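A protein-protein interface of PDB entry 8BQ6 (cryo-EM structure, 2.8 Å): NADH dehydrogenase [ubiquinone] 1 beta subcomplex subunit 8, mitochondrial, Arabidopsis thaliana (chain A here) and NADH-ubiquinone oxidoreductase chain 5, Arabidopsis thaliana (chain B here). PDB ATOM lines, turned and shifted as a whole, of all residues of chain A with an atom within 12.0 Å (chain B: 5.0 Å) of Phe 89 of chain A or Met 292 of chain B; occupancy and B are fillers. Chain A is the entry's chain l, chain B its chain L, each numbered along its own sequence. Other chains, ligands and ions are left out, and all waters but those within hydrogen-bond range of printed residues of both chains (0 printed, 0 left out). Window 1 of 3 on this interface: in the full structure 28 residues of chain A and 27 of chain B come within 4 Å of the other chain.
Printed residues of chain B within 4 Å of Gly 85 of chain A: Trp 563 (3.6 Å). Printed residues of chain B within 4 Å of Phe 88 of chain A: Phe 295 (3.6 Å). Phe 89 of chain A touches just these residues of chain B: Met 292, Phe 295, Phe 418, Leu 422 and Trp 563. Printed residues of chain B within 4 Å of Leu 92 of chain A: Phe 418 (3.6 Å) and Leu 422 (3.6 Å). Printed residues of chain B within 4 Å of Gly 93 of chain A: Phe 418. No residue of chain A comes within 4 Å of Ile 236 of chain B. No residue of chain A comes within 4 Å of Phe 288 of chain B. Gly 290 of chain B touches none of the printed residues of chain A. Of chain A, only Phe 89 comes within 4 Å of Met 292 of chain B. No residue of chain A comes within 4 Å of Ser 294 of chain B. Leu 422 of chain B touches two residues of chain A. Printed residues of chain A within 4 Å of Trp 563 of chain B: Leu 82, Gly 85 and Phe 89. The nearest residue of chain A that does not touch Met 292 of chain B is Leu 86 of chain A (6.1 Å). The nearest printed residue of chain B that does not touch Phe 88 of chain A is Leu 422 of chain B (4.5 Å).
Among the printed residues, merely in contact across the chains: Leu 82 of chain A with Trp 563 of chain B, Gly 85 of chain A with Trp 563 of chain B, Phe 88 of chain A with Phe 295 of chain B, Leu 92 of chain A with Leu 422 of chain B, Leu 92 of chain A with Phe 418 of chain B, Phe 89 of chain A with Met 292 of chain B, Phe 89 of chain A with Phe 418 of chain B, Phe 89 of chain A with Trp 563 of chain B, Phe 89 of chain A with Phe 295 of chain B, Gly 93 of chain A with Phe 418 of chain B and Phe 89 of chain A with Leu 422 of chain B.
Hydrophobic or aromatic side chains of chain A within 4 Å of the printed part of chain B: Leu 82, Phe 88, Phe 89 and Leu 92. Of the 13 printed residues of chain B, 5 touch a printed residue of chain A. Printed residues of chain B that touch a printed residue of chain A: Met 292, Phe 295, Phe 418, Leu 422 and Trp 563. Along chain B the printed residues that touch a printed residue of chain A span positions 292 to 563. Among the printed residues, 11 pairs touch across the chains. Among the printed residues, no Asp or Glu carboxylate lies within 4 Å of a Lys or Arg side-chain nitrogen of the other chain.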
ATOM      1  N   ALA A  80      26.822  -9.454  13.433  1.00  0.00           N
ATOM      2  CA  ALA A  80      27.396  -9.982  12.200  1.00  0.00           C
ATOM      3  C   ALA A  80      28.407 -11.086  12.490  1.00  0.00           C
ATOM      4  O   ALA A  80      28.494 -12.070  11.748  1.00  0.00           O
ATOM      5  CB  ALA A  80      28.036  -8.856  11.390  1.00  0.00           C
ATOM      6  N   TRP A  81      29.190 -10.939  13.561  1.00  0.00           N
ATOM      7  CA  TRP A  81      30.157 -11.978  13.903  1.00  0.00           C
ATOM      8  C   TRP A  81      29.456 -13.237  14.392  1.00  0.00           C
ATOM      9  O   TRP A  81      29.847 -14.355  14.043  1.00  0.00           O
ATOM     10  CB  TRP A  81      31.136 -11.471  14.956  1.00  0.00           C
ATOM     11  CG  TRP A  81      32.273 -10.725  14.377  1.00  0.00           C
ATOM     12  CD1 TRP A  81      32.306  -9.401  14.073  1.00  0.00           C
ATOM     13  CD2 TRP A  81      33.556 -11.252  14.023  1.00  0.00           C
ATOM     14  NE1 TRP A  81      33.528  -9.064  13.554  1.00  0.00           N
ATOM     15  CE2 TRP A  81      34.316 -10.184  13.512  1.00  0.00           C
ATOM     16  CE3 TRP A  81      34.136 -12.521  14.092  1.00  0.00           C
ATOM     17  CZ2 TRP A  81      35.623 -10.345  13.071  1.00  0.00           C
ATOM     18  CZ3 TRP A  81      35.435 -12.679  13.653  1.00  0.00           C
ATOM     19  CH2 TRP A  81      36.163 -11.597  13.149  1.00  0.00           C
ATOM     20  N   LEU A  82      28.421 -13.068  15.218  1.00  0.00           N
ATOM     21  CA  LEU A  82      27.639 -14.245  15.685  1.00  0.00           C
ATOM     22  C   LEU A  82      26.921 -14.876  14.488  1.00  0.00           C
ATOM     23  O   LEU A  82      26.871 -16.113  14.429  1.00  0.00           O
ATOM     24  CB  LEU A  82      26.642 -13.831  16.771  1.00  0.00           C
ATOM     25  CG  LEU A  82      25.689 -14.933  17.241  1.00  0.00           C
ATOM     26  CD1 LEU A  82      26.450 -16.141  17.762  1.00  0.00           C
ATOM     27  CD2 LEU A  82      24.726 -14.418  18.295  1.00  0.00           C
ATOM     28  N   SER A  83      26.405 -14.056  13.570  1.00  0.00           N
ATOM     29  CA  SER A  83      25.734 -14.598  12.392  1.00  0.00           C
ATOM     30  C   SER A  83      26.690 -15.430  11.546  1.00  0.00           C
ATOM     31  O   SER A  83      26.308 -16.478  11.012  1.00  0.00           O
ATOM     32  CB  SER A  83      25.138 -13.467  11.558  1.00  0.00           C
ATOM     33  OG  SER A  83      24.084 -13.939  10.741  1.00  0.00           O
ATOM     34  N   GLY A  84      27.931 -14.968  11.396  1.00  0.00           N
ATOM     35  CA  GLY A  84      28.920 -15.760  10.688  1.00  0.00           C
ATOM     36  C   GLY A  84      29.232 -17.065  11.397  1.00  0.00           C
ATOM     37  O   GLY A  84      29.346 -18.115  10.763  1.00  0.00           O
ATOM     38  N   GLY A  85      29.376 -17.013  12.723  1.00  0.00           N
ATOM     39  CA  GLY A  85      29.607 -18.233  13.478  1.00  0.00           C
ATOM     40  C   GLY A  85      28.488 -19.240  13.300  1.00  0.00           C
ATOM     41  O   GLY A  85      28.734 -20.435  13.127  1.00  0.00           O
ATOM     42  N   LEU A  86      27.241 -18.769  13.331  1.00  0.00           N
ATOM     43  CA  LEU A  86      26.121 -19.661  13.057  1.00  0.00           C
ATOM     44  C   LEU A  86      26.062 -20.037  11.581  1.00  0.00           C
ATOM     45  O   LEU A  86      25.512 -21.088  11.232  1.00  0.00           O
ATOM     46  CB  LEU A  86      24.817 -19.013  13.518  1.00  0.00           C
ATOM     47  CG  LEU A  86      24.745 -18.767  15.032  1.00  0.00           C
ATOM     48  CD1 LEU A  86      23.356 -18.332  15.467  1.00  0.00           C
ATOM     49  CD2 LEU A  86      25.186 -19.997  15.814  1.00  0.00           C
ATOM     50  N   GLY A  87      26.634 -19.206  10.706  1.00  0.00           N
ATOM     51  CA  GLY A  87      26.729 -19.575   9.304  1.00  0.00           C
ATOM     52  C   GLY A  87      27.769 -20.645   9.048  1.00  0.00           C
ATOM     53  O   GLY A  87      27.789 -21.253   7.974  1.00  0.00           O
ATOM     54  N   PHE A  88      28.651 -20.883  10.015  1.00  0.00           N
ATOM     55  CA  PHE A  88      29.577 -22.000   9.895  1.00  0.00           C
ATOM     56  C   PHE A  88      28.846 -23.324  10.085  1.00  0.00           C
ATOM     57  O   PHE A  88      29.059 -24.281   9.329  1.00  0.00           O
ATOM     58  CB  PHE A  88      30.709 -21.845  10.905  1.00  0.00           C
ATOM     59  CG  PHE A  88      31.528 -23.075  11.073  1.00  0.00           C
ATOM     60  CD1 PHE A  88      32.238 -23.597  10.009  1.00  0.00           C
ATOM     61  CD2 PHE A  88      31.576 -23.725  12.290  1.00  0.00           C
ATOM     62  CE1 PHE A  88      32.988 -24.738  10.160  1.00  0.00           C
ATOM     63  CE2 PHE A  88      32.323 -24.864  12.449  1.00  0.00           C
ATOM     64  CZ  PHE A  88      33.030 -25.374  11.385  1.00  0.00           C
ATOM     65  N   PHE A  89      27.960 -23.390  11.085  1.00  0.00           N
ATOM     66  CA  PHE A  89      27.142 -24.583  11.287  1.00  0.00           C
ATOM     67  C   PHE A  89      26.234 -24.837  10.094  1.00  0.00           C
ATOM     68  O   PHE A  89      25.957 -25.991   9.748  1.00  0.00           O
ATOM     69  CB  PHE A  89      26.296 -24.443  12.553  1.00  0.00           C
ATOM     70  CG  PHE A  89      27.091 -24.409  13.822  1.00  0.00           C
ATOM     71  CD1 PHE A  89      28.183 -25.237  13.994  1.00  0.00           C
ATOM     72  CD2 PHE A  89      26.733 -23.558  14.851  1.00  0.00           C
ATOM     73  CE1 PHE A  89      28.906 -25.207  15.162  1.00  0.00           C
ATOM     74  CE2 PHE A  89      27.454 -23.528  16.022  1.00  0.00           C
ATOM     75  CZ  PHE A  89      28.542 -24.352  16.176  1.00  0.00           C
ATOM     76  N   VAL A  90      25.725 -23.767   9.480  1.00  0.00           N
ATOM     77  CA  VAL A  90      24.850 -23.915   8.320  1.00  0.00           C
ATOM     78  C   VAL A  90      25.619 -24.509   7.146  1.00  0.00           C
ATOM     79  O   VAL A  90      25.154 -25.451   6.493  1.00  0.00           O
ATOM     80  CB  VAL A  90      24.215 -22.558   7.961  1.00  0.00           C
ATOM     81  CG1 VAL A  90      23.898 -22.481   6.477  1.00  0.00           C
ATOM     82  CG2 VAL A  90      22.962 -22.329   8.786  1.00  0.00           C
ATOM     83  N   GLY A  91      26.811 -23.978   6.867  1.00  0.00           N
ATOM     84  CA  GLY A  91      27.612 -24.511   5.777  1.00  0.00           C
ATOM     85  C   GLY A  91      28.108 -25.919   6.048  1.00  0.00           C
ATOM     86  O   GLY A  91      28.165 -26.753   5.142  1.00  0.00           O
ATOM     87  N   LEU A  92      28.490 -26.196   7.296  1.00  0.00           N
ATOM     88  CA  LEU A  92      28.883 -27.551   7.669  1.00  0.00           C
ATOM     89  C   LEU A  92      27.728 -28.525   7.491  1.00  0.00           C
ATOM     90  O   LEU A  92      27.920 -29.641   6.994  1.00  0.00           O
ATOM     91  CB  LEU A  92      29.382 -27.567   9.114  1.00  0.00           C
ATOM     92  CG  LEU A  92      30.300 -28.685   9.613  1.00  0.00           C
ATOM     93  CD1 LEU A  92      30.869 -28.290  10.956  1.00  0.00           C
ATOM     94  CD2 LEU A  92      29.570 -30.010   9.744  1.00  0.00           C
ATOM     95  N   GLY A  93      26.523 -28.129   7.903  1.00  0.00           N
ATOM     96  CA  GLY A  93      25.371 -28.995   7.714  1.00  0.00           C
ATOM     97  C   GLY A  93      25.074 -29.258   6.250  1.00  0.00           C
ATOM     98  O   GLY A  93      24.722 -30.378   5.871  1.00  0.00           O
ATOM     99  N   LEU A  94      25.197 -28.224   5.410  1.00  0.00           N
ATOM    100  CA  LEU A  94      25.017 -28.403   3.971  1.00  0.00           C
ATOM    101  C   LEU A  94      26.069 -29.343   3.401  1.00  0.00           C
ATOM    102  O   LEU A  94      25.762 -30.193   2.559  1.00  0.00           O
ATOM    103  CB  LEU A  94      25.081 -27.052   3.257  1.00  0.00           C
ATOM    104  CG  LEU A  94      23.970 -26.026   3.486  1.00  0.00           C
ATOM    105  CD1 LEU A  94      23.911 -25.040   2.330  1.00  0.00           C
ATOM    106  CD2 LEU A  94      22.634 -26.714   3.670  1.00  0.00           C
ATOM    107  N   LEU A  95      27.317 -29.193   3.849  1.00  0.00           N
ATOM    108  CA  LEU A  95      28.384 -30.095   3.429  1.00  0.00           C
ATOM    109  C   LEU A  95      28.059 -31.535   3.803  1.00  0.00           C
ATOM    110  O   LEU A  95      28.430 -32.471   3.085  1.00  0.00           O
ATOM    111  CB  LEU A  95      29.701 -29.655   4.064  1.00  0.00           C
ATOM    112  CG  LEU A  95      31.031 -30.038   3.420  1.00  0.00           C
ATOM    113  CD1 LEU A  95      31.323 -29.124   2.246  1.00  0.00           C
ATOM    114  CD2 LEU A  95      32.146 -29.964   4.453  1.00  0.00           C
ATOM    115  N   ALA A  96      27.366 -31.733   4.927  1.00  0.00           N
ATOM    116  CA  ALA A  96      26.969 -33.079   5.322  1.00  0.00           C
ATOM    117  C   ALA A  96      25.924 -33.649   4.371  1.00  0.00           C
ATOM    118  O   ALA A  96      25.922 -34.853   4.092  1.00  0.00           O
ATOM    119  CB  ALA A  96      26.445 -33.076   6.757  1.00  0.00           C
ATOM    120  N   VAL A  97      25.016 -32.802   3.881  1.00  0.00           N
ATOM    121  CA  VAL A  97      24.065 -33.232   2.861  1.00  0.00           C
ATOM    122  C   VAL A  97      24.796 -33.548   1.563  1.00  0.00           C
ATOM    123  O   VAL A  97      24.552 -34.577   0.921  1.00  0.00           O
ATOM    124  CB  VAL A  97      22.992 -32.150   2.645  1.00  0.00           C
ATOM    125  CG1 VAL A  97      22.241 -32.399   1.350  1.00  0.00           C
ATOM    126  CG2 VAL A  97      22.045 -32.090   3.829  1.00  0.00           C
ATOM    127  N   LEU A  98      25.711 -32.664   1.161  1.00  0.00           N
ATOM    128  CA  LEU A  98      26.458 -32.876  -0.071  1.00  0.00           C
ATOM    129  C   LEU A  98      27.308 -34.136  -0.002  1.00  0.00           C
ATOM    130  O   LEU A  98      27.508 -34.803  -1.023  1.00  0.00           O
ATOM    131  CB  LEU A  98      27.333 -31.660  -0.365  1.00  0.00           C
ATOM    132  CG  LEU A  98      26.666 -30.519  -1.129  1.00  0.00           C
ATOM    133  CD1 LEU A  98      27.712 -29.716  -1.872  1.00  0.00           C
ATOM    134  CD2 LEU A  98      25.616 -31.059  -2.086  1.00  0.00           C
ATOM    135  N   ILE B 236      23.105 -25.220  23.065  1.00  0.00           N
ATOM    136  CA  ILE B 236      23.118 -23.990  22.218  1.00  0.00           C
ATOM    137  C   ILE B 236      21.731 -23.332  22.235  1.00  0.00           C
ATOM    138  O   ILE B 236      20.721 -24.036  22.038  1.00  0.00           O
ATOM    139  CB  ILE B 236      23.614 -24.305  20.789  1.00  0.00           C
ATOM    140  CG1 ILE B 236      23.639 -23.054  19.908  1.00  0.00           C
ATOM    141  CG2 ILE B 236      22.810 -25.430  20.153  1.00  0.00           C
ATOM    142  CD1 ILE B 236      24.292 -23.263  18.564  1.00  0.00           C
ATOM    143  N   PHE B 288      21.711 -32.536  16.263  1.00  0.00           N
ATOM    144  CA  PHE B 288      22.328 -31.274  15.861  1.00  0.00           C
ATOM    145  C   PHE B 288      22.647 -30.395  17.063  1.00  0.00           C
ATOM    146  O   PHE B 288      23.701 -29.749  17.105  1.00  0.00           O
ATOM    147  CB  PHE B 288      21.415 -30.528  14.891  1.00  0.00           C
ATOM    148  CG  PHE B 288      21.572 -30.946  13.460  1.00  0.00           C
ATOM    149  CD1 PHE B 288      22.685 -30.567  12.729  1.00  0.00           C
ATOM    150  CD2 PHE B 288      20.606 -31.716  12.843  1.00  0.00           C
ATOM    151  CE1 PHE B 288      22.826 -30.954  11.409  1.00  0.00           C
ATOM    152  CE2 PHE B 288      20.745 -32.104  11.527  1.00  0.00           C
ATOM    153  CZ  PHE B 288      21.853 -31.721  10.809  1.00  0.00           C
ATOM    154  N   ALA B 289      21.738 -30.347  18.039  1.00  0.00           N
ATOM    155  CA  ALA B 289      21.937 -29.481  19.224  1.00  0.00           C
ATOM    156  C   ALA B 289      23.224 -29.876  19.951  1.00  0.00           C
ATOM    157  O   ALA B 289      24.117 -29.020  20.071  1.00  0.00           O
ATOM    158  CB  ALA B 289      20.756 -29.591  20.141  1.00  0.00           C
ATOM    159  N   GLY B 290      23.294 -31.111  20.434  1.00  0.00           N
ATOM    160  CA  GLY B 290      24.489 -31.587  21.147  1.00  0.00           C
ATOM    161  C   GLY B 290      25.762 -31.335  20.364  1.00  0.00           C
ATOM    162  O   GLY B 290      26.704 -30.790  20.960  1.00  0.00           O
ATOM    163  N   ALA B 291      25.787 -31.674  19.073  1.00  0.00           N
ATOM    164  CA  ALA B 291      27.020 -31.546  18.302  1.00  0.00           C
ATOM    165  C   ALA B 291      27.484 -30.097  18.235  1.00  0.00           C
ATOM    166  O   ALA B 291      28.675 -29.808  18.399  1.00  0.00           O
ATOM    167  CB  ALA B 291      26.821 -32.110  16.896  1.00  0.00           C
ATOM    168  N   MET B 292      26.556 -29.169  17.981  1.00  0.00           N
ATOM    169  CA  MET B 292      26.929 -27.758  17.921  1.00  0.00           C
ATOM    170  C   MET B 292      27.412 -27.254  19.271  1.00  0.00           C
ATOM    171  O   MET B 292      28.377 -26.486  19.346  1.00  0.00           O
ATOM    172  CB  MET B 292      25.754 -26.909  17.438  1.00  0.00           C
ATOM    173  CG  MET B 292      25.317 -27.193  16.021  1.00  0.00           C
ATOM    174  SD  MET B 292      24.077 -26.024  15.430  1.00  0.00           S
ATOM    175  CE  MET B 292      22.562 -26.795  15.987  1.00  0.00           C
ATOM    176  N   THR B 293      26.729 -27.662  20.337  1.00  0.00           N
ATOM    177  CA  THR B 293      27.104 -27.213  21.701  1.00  0.00           C
ATOM    178  C   THR B 293      28.542 -27.637  22.001  1.00  0.00           C
ATOM    179  O   THR B 293      29.306 -26.792  22.502  1.00  0.00           O
ATOM    180  CB  THR B 293      26.150 -27.778  22.757  1.00  0.00           C
ATOM    181  OG1 THR B 293      24.815 -27.473  22.357  1.00  0.00           O
ATOM    182  CG2 THR B 293      26.409 -27.229  24.142  1.00  0.00           C
ATOM    183  N   SER B 294      28.891 -28.889  21.714  1.00  0.00           N
ATOM    184  CA  SER B 294      30.225 -29.383  22.037  1.00  0.00           C
ATOM    185  C   SER B 294      31.303 -28.534  21.376  1.00  0.00           C
ATOM    186  O   SER B 294      32.362 -28.292  21.966  1.00  0.00           O
ATOM    187  CB  SER B 294      30.359 -30.846  21.618  1.00  0.00           C
ATOM    188  OG  SER B 294      30.096 -31.009  20.236  1.00  0.00           O
ATOM    189  N   PHE B 295      31.050 -28.075  20.152  1.00  0.00           N
ATOM    190  CA  PHE B 295      32.003 -27.212  19.465  1.00  0.00           C
ATOM    191  C   PHE B 295      31.979 -25.797  20.034  1.00  0.00           C
ATOM    192  O   PHE B 295      33.032 -25.167  20.194  1.00  0.00           O
ATOM    193  CB  PHE B 295      31.690 -27.213  17.971  1.00  0.00           C
ATOM    194  CG  PHE B 295      32.680 -26.467  17.138  1.00  0.00           C
ATOM    195  CD1 PHE B 295      33.899 -27.031  16.809  1.00  0.00           C
ATOM    196  CD2 PHE B 295      32.384 -25.205  16.665  1.00  0.00           C
ATOM    197  CE1 PHE B 295      34.805 -26.342  16.031  1.00  0.00           C
ATOM    198  CE2 PHE B 295      33.285 -24.514  15.891  1.00  0.00           C
ATOM    199  CZ  PHE B 295      34.498 -25.083  15.572  1.00  0.00           C
ATOM    200  N   LEU B 296      30.782 -25.279  20.329  1.00  0.00           N
ATOM    201  CA  LEU B 296      30.638 -23.886  20.837  1.00  0.00           C
ATOM    202  C   LEU B 296      31.354 -23.733  22.184  1.00  0.00           C
ATOM    203  O   LEU B 296      32.011 -22.702  22.366  1.00  0.00           O
ATOM    204  CB  LEU B 296      29.152 -23.539  20.970  1.00  0.00           C
ATOM    205  CG  LEU B 296      28.837 -22.162  21.550  1.00  0.00           C
ATOM    206  CD1 LEU B 296      29.368 -21.068  20.644  1.00  0.00           C
ATOM    207  CD2 LEU B 296      27.344 -21.980  21.777  1.00  0.00           C
ATOM    208  N   PHE B 418      27.199 -34.983  10.744  1.00  0.00           N
ATOM    209  CA  PHE B 418      27.380 -33.682  11.370  1.00  0.00           C
ATOM    210  C   PHE B 418      27.995 -33.828  12.757  1.00  0.00           C
ATOM    211  O   PHE B 418      28.910 -33.083  13.130  1.00  0.00           O
ATOM    212  CB  PHE B 418      26.028 -32.975  11.436  1.00  0.00           C
ATOM    213  CG  PHE B 418      26.096 -31.587  11.967  1.00  0.00           C
ATOM    214  CD1 PHE B 418      26.270 -30.521  11.105  1.00  0.00           C
ATOM    215  CD2 PHE B 418      25.954 -31.338  13.317  1.00  0.00           C
ATOM    216  CE1 PHE B 418      26.326 -29.236  11.581  1.00  0.00           C
ATOM    217  CE2 PHE B 418      26.007 -30.054  13.797  1.00  0.00           C
ATOM    218  CZ  PHE B 418      26.193 -29.000  12.925  1.00  0.00           C
ATOM    219  N   LEU B 422      31.946 -32.671  14.166  1.00  0.00           N
ATOM    220  CA  LEU B 422      32.014 -31.657  15.213  1.00  0.00           C
ATOM    221  C   LEU B 422      32.490 -32.248  16.534  1.00  0.00           C
ATOM    222  O   LEU B 422      33.194 -31.581  17.301  1.00  0.00           O
ATOM    223  CB  LEU B 422      30.650 -30.994  15.374  1.00  0.00           C
ATOM    224  CG  LEU B 422      30.423 -29.825  14.418  1.00  0.00           C
ATOM    225  CD1 LEU B 422      29.172 -29.076  14.795  1.00  0.00           C
ATOM    226  CD2 LEU B 422      31.621 -28.893  14.427  1.00  0.00           C
ATOM    227  N   TRP B 563      31.325 -15.883  21.326  1.00  0.00           N
ATOM    228  CA  TRP B 563      30.574 -15.669  20.056  1.00  0.00           C
ATOM    229  C   TRP B 563      29.597 -14.496  20.209  1.00  0.00           C
ATOM    230  O   TRP B 563      28.598 -14.487  19.484  1.00  0.00           O
ATOM    231  CB  TRP B 563      29.852 -16.953  19.626  1.00  0.00           C
ATOM    232  CG  TRP B 563      30.722 -18.153  19.400  1.00  0.00           C
ATOM    233  CD1 TRP B 563      31.815 -18.542  20.121  1.00  0.00           C
ATOM    234  CD2 TRP B 563      30.544 -19.158  18.386  1.00  0.00           C
ATOM    235  NE1 TRP B 563      32.338 -19.701  19.616  1.00  0.00           N
ATOM    236  CE2 TRP B 563      31.579 -20.103  18.552  1.00  0.00           C
ATOM    237  CE3 TRP B 563      29.621 -19.346  17.352  1.00  0.00           C
ATOM    238  CZ2 TRP B 563      31.711 -21.215  17.722  1.00  0.00           C
ATOM    239  CZ3 TRP B 563      29.753 -20.444  16.534  1.00  0.00           C
ATOM    240  CH2 TRP B 563      30.785 -21.362  16.716  1.00  0.00           C
